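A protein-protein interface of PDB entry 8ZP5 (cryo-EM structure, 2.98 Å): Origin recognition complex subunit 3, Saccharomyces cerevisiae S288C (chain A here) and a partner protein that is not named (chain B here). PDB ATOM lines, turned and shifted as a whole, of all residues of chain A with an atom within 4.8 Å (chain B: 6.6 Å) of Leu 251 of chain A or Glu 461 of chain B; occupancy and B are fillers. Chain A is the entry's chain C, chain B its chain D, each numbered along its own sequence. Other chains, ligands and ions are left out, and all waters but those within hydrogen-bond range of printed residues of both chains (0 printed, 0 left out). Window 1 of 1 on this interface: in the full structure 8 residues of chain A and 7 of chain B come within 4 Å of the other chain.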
ATOM      1  N   PHE A 213     -16.375 -21.116 -20.378  1.00  0.00           N
ATOM      2  CA  PHE A 213     -15.902 -19.798 -20.772  1.00  0.00           C
ATOM      3  C   PHE A 213     -16.706 -18.671 -20.144  1.00  0.00           C
ATOM      4  O   PHE A 213     -16.205 -17.546 -20.064  1.00  0.00           O
ATOM      5  CB  PHE A 213     -15.913 -19.674 -22.294  1.00  0.00           C
ATOM      6  CG  PHE A 213     -14.756 -20.360 -22.956  1.00  0.00           C
ATOM      7  CD1 PHE A 213     -13.496 -19.791 -22.937  1.00  0.00           C
ATOM      8  CD2 PHE A 213     -14.925 -21.582 -23.583  1.00  0.00           C
ATOM      9  CE1 PHE A 213     -12.428 -20.420 -23.540  1.00  0.00           C
ATOM     10  CE2 PHE A 213     -13.860 -22.216 -24.190  1.00  0.00           C
ATOM     11  CZ  PHE A 213     -12.610 -21.635 -24.166  1.00  0.00           C
ATOM     12  N   ASP A 217     -14.613 -15.882 -18.321  1.00  0.00           N
ATOM     13  CA  ASP A 217     -14.776 -14.480 -18.689  1.00  0.00           C
ATOM     14  C   ASP A 217     -15.122 -13.631 -17.473  1.00  0.00           C
ATOM     15  O   ASP A 217     -14.584 -12.529 -17.299  1.00  0.00           O
ATOM     16  CB  ASP A 217     -15.855 -14.352 -19.762  1.00  0.00           C
ATOM     17  CG  ASP A 217     -15.746 -13.065 -20.550  1.00  0.00           C
ATOM     18  OD1 ASP A 217     -15.084 -12.125 -20.067  1.00  0.00           O
ATOM     19  OD2 ASP A 217     -16.324 -12.994 -21.654  1.00  0.00           O
ATOM     20  N   ILE A 247     -11.642 -19.471 -28.581  1.00  0.00           N
ATOM     21  CA  ILE A 247     -11.708 -18.571 -27.436  1.00  0.00           C
ATOM     22  C   ILE A 247     -12.300 -17.227 -27.843  1.00  0.00           C
ATOM     23  O   ILE A 247     -13.072 -16.622 -27.090  1.00  0.00           O
ATOM     24  CB  ILE A 247     -10.315 -18.424 -26.800  1.00  0.00           C
ATOM     25  CG1 ILE A 247      -9.946 -19.706 -26.057  1.00  0.00           C
ATOM     26  CG2 ILE A 247     -10.258 -17.233 -25.869  1.00  0.00           C
ATOM     27  CD1 ILE A 247      -8.576 -19.677 -25.464  1.00  0.00           C
ATOM     28  N   GLU A 248     -11.958 -16.742 -29.039  1.00  0.00           N
ATOM     29  CA  GLU A 248     -12.552 -15.501 -29.524  1.00  0.00           C
ATOM     30  C   GLU A 248     -14.065 -15.627 -29.647  1.00  0.00           C
ATOM     31  O   GLU A 248     -14.805 -14.707 -29.284  1.00  0.00           O
ATOM     32  CB  GLU A 248     -11.941 -15.112 -30.870  1.00  0.00           C
ATOM     33  CG  GLU A 248     -10.548 -14.520 -30.777  1.00  0.00           C
ATOM     34  CD  GLU A 248     -10.102 -13.889 -32.080  1.00  0.00           C
ATOM     35  OE1 GLU A 248     -10.825 -14.032 -33.088  1.00  0.00           O
ATOM     36  OE2 GLU A 248      -9.030 -13.252 -32.099  1.00  0.00           O
ATOM     37  N   LYS A 249     -14.542 -16.760 -30.163  1.00  0.00           N
ATOM     38  CA  LYS A 249     -15.981 -16.970 -30.281  1.00  0.00           C
ATOM     39  C   LYS A 249     -16.641 -17.149 -28.920  1.00  0.00           C
ATOM     40  O   LYS A 249     -17.804 -16.769 -28.744  1.00  0.00           O
ATOM     41  CB  LYS A 249     -16.265 -18.182 -31.166  1.00  0.00           C
ATOM     42  CG  LYS A 249     -16.581 -17.841 -32.613  1.00  0.00           C
ATOM     43  CD  LYS A 249     -15.311 -17.643 -33.423  1.00  0.00           C
ATOM     44  CE  LYS A 249     -15.619 -17.452 -34.898  1.00  0.00           C
ATOM     45  NZ  LYS A 249     -14.516 -16.741 -35.604  1.00  0.00           N
ATOM     46  N   ASN A 250     -15.929 -17.723 -27.952  1.00  0.00           N
ATOM     47  CA  ASN A 250     -16.502 -18.047 -26.653  1.00  0.00           C
ATOM     48  C   ASN A 250     -16.322 -16.949 -25.613  1.00  0.00           C
ATOM     49  O   ASN A 250     -16.815 -17.096 -24.491  1.00  0.00           O
ATOM     50  CB  ASN A 250     -15.899 -19.353 -26.127  1.00  0.00           C
ATOM     51  CG  ASN A 250     -16.242 -20.545 -26.996  1.00  0.00           C
ATOM     52  OD1 ASN A 250     -17.357 -20.656 -27.505  1.00  0.00           O
ATOM     53  ND2 ASN A 250     -15.281 -21.443 -27.174  1.00  0.00           N
ATOM     54  N   LEU A 251     -15.635 -15.860 -25.944  1.00  0.00           N
ATOM     55  CA  LEU A 251     -15.451 -14.750 -25.021  1.00  0.00           C
ATOM     56  C   LEU A 251     -16.188 -13.514 -25.517  1.00  0.00           C
ATOM     57  O   LEU A 251     -16.388 -13.328 -26.720  1.00  0.00           O
ATOM     58  CB  LEU A 251     -13.970 -14.410 -24.828  1.00  0.00           C
ATOM     59  CG  LEU A 251     -13.105 -15.349 -23.989  1.00  0.00           C
ATOM     60  CD1 LEU A 251     -11.718 -14.755 -23.825  1.00  0.00           C
ATOM     61  CD2 LEU A 251     -13.739 -15.613 -22.637  1.00  0.00           C
ATOM     62  N   ARG A 252     -16.591 -12.674 -24.570  1.00  0.00           N
ATOM     63  CA  ARG A 252     -17.235 -11.414 -24.907  1.00  0.00           C
ATOM     64  C   ARG A 252     -16.250 -10.485 -25.603  1.00  0.00           C
ATOM     65  O   ARG A 252     -15.038 -10.551 -25.383  1.00  0.00           O
ATOM     66  CB  ARG A 252     -17.790 -10.747 -23.650  1.00  0.00           C
ATOM     67  CG  ARG A 252     -18.947 -11.493 -23.016  1.00  0.00           C
ATOM     68  CD  ARG A 252     -19.685 -10.621 -22.017  1.00  0.00           C
ATOM     69  NE  ARG A 252     -18.975 -10.527 -20.748  1.00  0.00           N
ATOM     70  CZ  ARG A 252     -19.266 -11.248 -19.672  1.00  0.00           C
ATOM     71  NH1 ARG A 252     -20.247 -12.134 -19.679  1.00  0.00           N
ATOM     72  NH2 ARG A 252     -18.551 -11.075 -18.564  1.00  0.00           N
ATOM     73  N   GLN A 253     -16.783  -9.613 -26.462  1.00  0.00           N
ATOM     74  CA  GLN A 253     -15.926  -8.693 -27.200  1.00  0.00           C
ATOM     75  C   GLN A 253     -15.217  -7.716 -26.275  1.00  0.00           C
ATOM     76  O   GLN A 253     -14.105  -7.272 -26.580  1.00  0.00           O
ATOM     77  CB  GLN A 253     -16.740  -7.938 -28.248  1.00  0.00           C
ATOM     78  CG  GLN A 253     -16.976  -8.725 -29.521  1.00  0.00           C
ATOM     79  CD  GLN A 253     -15.691  -9.011 -30.268  1.00  0.00           C
ATOM     80  OE1 GLN A 253     -14.776  -8.188 -30.287  1.00  0.00           O
ATOM     81  NE2 GLN A 253     -15.615 -10.181 -30.889  1.00  0.00           N
ATOM     82  N   SER A 254     -15.840  -7.361 -25.149  1.00  0.00           N
ATOM     83  CA  SER A 254     -15.169  -6.501 -24.181  1.00  0.00           C
ATOM     84  C   SER A 254     -13.931  -7.181 -23.612  1.00  0.00           C
ATOM     85  O   SER A 254     -12.868  -6.559 -23.496  1.00  0.00           O
ATOM     86  CB  SER A 254     -16.134  -6.117 -23.060  1.00  0.00           C
ATOM     87  OG  SER A 254     -16.384  -7.217 -22.204  1.00  0.00           O
ATOM     88  N   THR A 255     -14.044  -8.465 -23.266  1.00  0.00           N
ATOM     89  CA  THR A 255     -12.888  -9.202 -22.769  1.00  0.00           C
ATOM     90  C   THR A 255     -11.837  -9.380 -23.857  1.00  0.00           C
ATOM     91  O   THR A 255     -10.635  -9.348 -23.576  1.00  0.00           O
ATOM     92  CB  THR A 255     -13.324 -10.558 -22.220  1.00  0.00           C
ATOM     93  OG1 THR A 255     -14.484 -10.389 -21.398  1.00  0.00           O
ATOM     94  CG2 THR A 255     -12.214 -11.175 -21.390  1.00  0.00           C
ATOM     95  N   ILE A 256     -12.271  -9.572 -25.103  1.00  0.00           N
ATOM     96  CA  ILE A 256     -11.324  -9.689 -26.208  1.00  0.00           C
ATOM     97  C   ILE A 256     -10.535  -8.398 -26.371  1.00  0.00           C
ATOM     98  O   ILE A 256      -9.309  -8.419 -26.534  1.00  0.00           O
ATOM     99  CB  ILE A 256     -12.061 -10.074 -27.503  1.00  0.00           C
ATOM    100  CG1 ILE A 256     -12.592 -11.504 -27.411  1.00  0.00           C
ATOM    101  CG2 ILE A 256     -11.146  -9.923 -28.699  1.00  0.00           C
ATOM    102  CD1 ILE A 256     -11.535 -12.524 -27.068  1.00  0.00           C
ATOM    103  N   LEU A 259      -8.039  -8.085 -23.525  1.00  0.00           N
ATOM    104  CA  LEU A 259      -6.871  -8.946 -23.684  1.00  0.00           C
ATOM    105  C   LEU A 259      -5.988  -8.497 -24.841  1.00  0.00           C
ATOM    106  O   LEU A 259      -4.783  -8.773 -24.839  1.00  0.00           O
ATOM    107  CB  LEU A 259      -7.311 -10.395 -23.893  1.00  0.00           C
ATOM    108  CG  LEU A 259      -7.992 -11.091 -22.715  1.00  0.00           C
ATOM    109  CD1 LEU A 259      -8.457 -12.481 -23.116  1.00  0.00           C
ATOM    110  CD2 LEU A 259      -7.060 -11.160 -21.519  1.00  0.00           C
ATOM    111  N   VAL B 456     -21.012  -7.626 -35.604  1.00  0.00           N
ATOM    112  CA  VAL B 456     -22.358  -7.662 -35.042  1.00  0.00           C
ATOM    113  C   VAL B 456     -22.418  -8.484 -33.760  1.00  0.00           C
ATOM    114  O   VAL B 456     -23.381  -8.340 -32.990  1.00  0.00           O
ATOM    115  CB  VAL B 456     -23.379  -8.175 -36.085  1.00  0.00           C
ATOM    116  CG1 VAL B 456     -24.762  -8.388 -35.498  1.00  0.00           C
ATOM    117  CG2 VAL B 456     -23.474  -7.195 -37.240  1.00  0.00           C
ATOM    118  N   LYS B 457     -21.397  -9.296 -33.477  1.00  0.00           N
ATOM    119  CA  LYS B 457     -21.344 -10.005 -32.201  1.00  0.00           C
ATOM    120  C   LYS B 457     -21.313  -9.032 -31.027  1.00  0.00           C
ATOM    121  O   LYS B 457     -21.969  -9.260 -30.002  1.00  0.00           O
ATOM    122  CB  LYS B 457     -20.124 -10.924 -32.171  1.00  0.00           C
ATOM    123  CG  LYS B 457     -19.956 -11.705 -30.883  1.00  0.00           C
ATOM    124  CD  LYS B 457     -18.648 -12.479 -30.882  1.00  0.00           C
ATOM    125  CE  LYS B 457     -18.335 -13.038 -29.506  1.00  0.00           C
ATOM    126  NZ  LYS B 457     -16.966 -13.613 -29.434  1.00  0.00           N
ATOM    127  N   ASN B 458     -20.553  -7.942 -31.155  1.00  0.00           N
ATOM    128  CA  ASN B 458     -20.505  -6.944 -30.092  1.00  0.00           C
ATOM    129  C   ASN B 458     -21.865  -6.289 -29.885  1.00  0.00           C
ATOM    130  O   ASN B 458     -22.279  -6.049 -28.746  1.00  0.00           O
ATOM    131  CB  ASN B 458     -19.448  -5.890 -30.408  1.00  0.00           C
ATOM    132  CG  ASN B 458     -19.252  -4.907 -29.275  1.00  0.00           C
ATOM    133  OD1 ASN B 458     -19.087  -5.298 -28.122  1.00  0.00           O
ATOM    134  ND2 ASN B 458     -19.274  -3.620 -29.598  1.00  0.00           N
ATOM    135  N   VAL B 459     -22.569  -5.983 -30.977  1.00  0.00           N
ATOM    136  CA  VAL B 459     -23.906  -5.405 -30.866  1.00  0.00           C
ATOM    137  C   VAL B 459     -24.856  -6.386 -30.194  1.00  0.00           C
ATOM    138  O   VAL B 459     -25.696  -6.000 -29.372  1.00  0.00           O
ATOM    139  CB  VAL B 459     -24.413  -4.979 -32.256  1.00  0.00           C
ATOM    140  CG1 VAL B 459     -25.922  -4.858 -32.264  1.00  0.00           C
ATOM    141  CG2 VAL B 459     -23.773  -3.669 -32.662  1.00  0.00           C
ATOM    142  N   TRP B 460     -24.738  -7.669 -30.534  1.00  0.00           N
ATOM    143  CA  TRP B 460     -25.562  -8.692 -29.900  1.00  0.00           C
ATOM    144  C   TRP B 460     -25.314  -8.737 -28.399  1.00  0.00           C
ATOM    145  O   TRP B 460     -26.256  -8.785 -27.598  1.00  0.00           O
ATOM    146  CB  TRP B 460     -25.269 -10.052 -30.534  1.00  0.00           C
ATOM    147  CG  TRP B 460     -26.307 -11.081 -30.265  1.00  0.00           C
ATOM    148  CD1 TRP B 460     -26.224 -12.118 -29.386  1.00  0.00           C
ATOM    149  CD2 TRP B 460     -27.590 -11.179 -30.884  1.00  0.00           C
ATOM    150  NE1 TRP B 460     -27.380 -12.858 -29.418  1.00  0.00           N
ATOM    151  CE2 TRP B 460     -28.236 -12.300 -30.331  1.00  0.00           C
ATOM    152  CE3 TRP B 460     -28.258 -10.425 -31.852  1.00  0.00           C
ATOM    153  CZ2 TRP B 460     -29.514 -12.686 -30.714  1.00  0.00           C
ATOM    154  CZ3 TRP B 460     -29.524 -10.808 -32.229  1.00  0.00           C
ATOM    155  CH2 TRP B 460     -30.140 -11.929 -31.663  1.00  0.00           C
ATOM    156  N   GLU B 461     -24.042  -8.712 -28.001  1.00  0.00           N
ATOM    157  CA  GLU B 461     -23.712  -8.744 -26.580  1.00  0.00           C
ATOM    158  C   GLU B 461     -24.208  -7.491 -25.869  1.00  0.00           C
ATOM    159  O   GLU B 461     -24.681  -7.563 -24.730  1.00  0.00           O
ATOM    160  CB  GLU B 461     -22.206  -8.912 -26.399  1.00  0.00           C
ATOM    161  CG  GLU B 461     -21.694 -10.266 -26.846  1.00  0.00           C
ATOM    162  CD  GLU B 461     -20.191 -10.299 -26.993  1.00  0.00           C
ATOM    163  OE1 GLU B 461     -19.566  -9.217 -26.967  1.00  0.00           O
ATOM    164  OE2 GLU B 461     -19.634 -11.406 -27.130  1.00  0.00           O
ATOM    165  N   ASN B 462     -24.104  -6.333 -26.523  1.00  0.00           N
ATOM    166  CA  ASN B 462     -24.593  -5.096 -25.923  1.00  0.00           C
ATOM    167  C   ASN B 462     -26.104  -5.133 -25.731  1.00  0.00           C
ATOM    168  O   ASN B 462     -26.615  -4.701 -24.693  1.00  0.00           O
ATOM    169  CB  ASN B 462     -24.190  -3.902 -26.785  1.00  0.00           C
ATOM    170  CG  ASN B 462     -22.716  -3.583 -26.680  1.00  0.00           C
ATOM    171  OD1 ASN B 462     -21.955  -4.311 -26.044  1.00  0.00           O
ATOM    172  ND2 ASN B 462     -22.302  -2.488 -27.305  1.00  0.00           N
ATOM    173  N   LEU B 463     -26.835  -5.639 -26.726  1.00  0.00           N
ATOM    174  CA  LEU B 463     -28.286  -5.741 -26.596  1.00  0.00           C
ATOM    175  C   LEU B 463     -28.681  -6.747 -25.526  1.00  0.00           C
ATOM    176  O   LEU B 463     -29.698  -6.561 -24.850  1.00  0.00           O
ATOM    177  CB  LEU B 463     -28.914  -6.119 -27.935  1.00  0.00           C
ATOM    178  CG  LEU B 463     -28.884  -5.061 -29.035  1.00  0.00           C
ATOM    179  CD1 LEU B 463     -29.185  -5.692 -30.379  1.00  0.00           C
ATOM    180  CD2 LEU B 463     -29.870  -3.952 -28.731  1.00  0.00           C
ATOM    181  N   VAL B 464     -27.905  -7.821 -25.367  1.00  0.00           N
ATOM    182  CA  VAL B 464     -28.179  -8.773 -24.295  1.00  0.00           C
ATOM    183  C   VAL B 464     -27.907  -8.139 -22.935  1.00  0.00           C
ATOM    184  O   VAL B 464     -28.634  -8.382 -21.965  1.00  0.00           O
ATOM    185  CB  VAL B 464     -27.359 -10.060 -24.506  1.00  0.00           C
ATOM    186  CG1 VAL B 464     -27.396 -10.933 -23.263  1.00  0.00           C
ATOM    187  CG2 VAL B 464     -27.886 -10.828 -25.705  1.00  0.00           C
ATOM    188  N   GLN B 465     -26.865  -7.307 -22.844  1.00  0.00           N
ATOM    189  CA  GLN B 465     -26.530  -6.664 -21.577  1.00  0.00           C
ATOM    190  C   GLN B 465     -27.647  -5.740 -21.108  1.00  0.00           C
ATOM    191  O   GLN B 465     -27.959  -5.691 -19.913  1.00  0.00           O
ATOM    192  CB  GLN B 465     -25.220  -5.889 -21.708  1.00  0.00           C
ATOM    193  CG  GLN B 465     -23.978  -6.741 -21.532  1.00  0.00           C
ATOM    194  CD  GLN B 465     -22.709  -5.916 -21.485  1.00  0.00           C
ATOM    195  OE1 GLN B 465     -22.755  -4.687 -21.455  1.00  0.00           O
ATOM    196  NE2 GLN B 465     -21.565  -6.590 -21.480  1.00  0.00           N
ATOM    197  N   LEU B 466     -28.259  -5.000 -22.029  1.00  0.00           N
ATOM    198  CA  LEU B 466     -29.384  -4.133 -21.703  1.00  0.00           C
ATOM    199  C   LEU B 466     -30.676  -4.907 -21.474  1.00  0.00           C
ATOM    200  O   LEU B 466     -31.735  -4.288 -21.330  1.00  0.00           O
ATOM    201  CB  LEU B 466     -29.594  -3.102 -22.815  1.00  0.00           C
ATOM    202  CG  LEU B 466     -28.391  -2.231 -23.179  1.00  0.00           C
ATOM    203  CD1 LEU B 466     -28.781  -1.186 -24.208  1.00  0.00           C
ATOM    204  CD2 LEU B 466     -27.813  -1.574 -21.942  1.00  0.00           C
ATOM    205  N   PHE B 499     -21.792 -19.677 -29.254  1.00  0.00           N
ATOM    206  CA  PHE B 499     -22.495 -18.403 -29.148  1.00  0.00           C
ATOM    207  C   PHE B 499     -23.496 -18.216 -30.282  1.00  0.00           C
ATOM    208  O   PHE B 499     -24.570 -17.635 -30.082  1.00  0.00           O
ATOM    209  CB  PHE B 499     -21.484 -17.257 -29.120  1.00  0.00           C
ATOM    210  CG  PHE B 499     -22.003 -15.974 -29.696  1.00  0.00           C
ATOM    211  CD1 PHE B 499     -22.848 -15.161 -28.963  1.00  0.00           C
ATOM    212  CD2 PHE B 499     -21.631 -15.573 -30.967  1.00  0.00           C
ATOM    213  CE1 PHE B 499     -23.324 -13.978 -29.490  1.00  0.00           C
ATOM    214  CE2 PHE B 499     -22.103 -14.392 -31.499  1.00  0.00           C
ATOM    215  CZ  PHE B 499     -22.950 -13.593 -30.759  1.00  0.00           C
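The side-chain carboxylate of Glu 461 of chain B is in hydrogen-bond range of the backbone NH of Gln 253 of chain A (2.9 Å).
The backbone carbonyl oxygen (O) of Lys 249 of chain A sits at hydrogen-bond distance from the side-chain amino group (NZ) of Lys 457 of chain B (3.3 Å).
The backbone carbonyl oxygen (O) of Leu 251 of chain A sits at hydrogen-bond distance from the side-chain amino group (NZ) of Lys 457 of chain B, 2.8 Å away.
The backbone carbonyl oxygen of Glu 248 of chain A is in hydrogen-bond range of the side-chain amino group of Lys 457 of chain B (2.4 Å).
The backbone carbonyl oxygen of Asn 458 of chain B lies close to the side-chain amide oxygen of Asn 462 of chain B (3.2 Å).
The guanidinium group (NE) of Arg 252 of chain A is in salt-bridge range of the side-chain carboxylate (OD2) of Asp 217 of chain A (3.7 Å).
O of Lys 249 of chain A touches CB of Phe 499 of chain B (3.7 Å).
Leu 251 of chain A touches Glu 461 of chain B (O to OE2, 3.8 Å).
CA of Arg 252 of chain A touches OE2 of Glu 461 of chain B, at 3.3 Å.
Lys 457 of chain B touches Gln 253 of chain A.
Gln 253 of chain A touches Asn 458 of chain B (CB to OD1, 3.5 Å).
Of chain B, only Lys 457 (2.8 Å) and Glu 461 (3.8 Å) come within 4 Å of Leu 251 of chain A.
Printed residues of chain A within 4 Å of Lys 457 of chain B: Glu 248 (2.4 Å), Lys 249 (3.3 Å), Leu 251 (2.8 Å) and Gln 253 (3.8 Å).
Glu 461 of chain B touches just these residues of chain A: Leu 251, Arg 252 and Gln 253.
Asn 462 of chain B touches none of the printed residues of chain A.
Val 464 of chain B touches none of the printed residues of chain A.
Of the printed residues of chain A, Phe 499 of chain B touches Lys 249.
The nearest printed residue of chain B that does not touch Leu 251 of chain A is Phe 499 of chain B (6.8 Å).
Printed residues of chain B that touch a printed residue of chain A: Lys 457, Asn 458, Glu 461 and Phe 499.
Of the 13 printed residues of chain A, 5 touch a printed residue of chain B.
Among the printed residues, 9 pairs touch across the chains.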
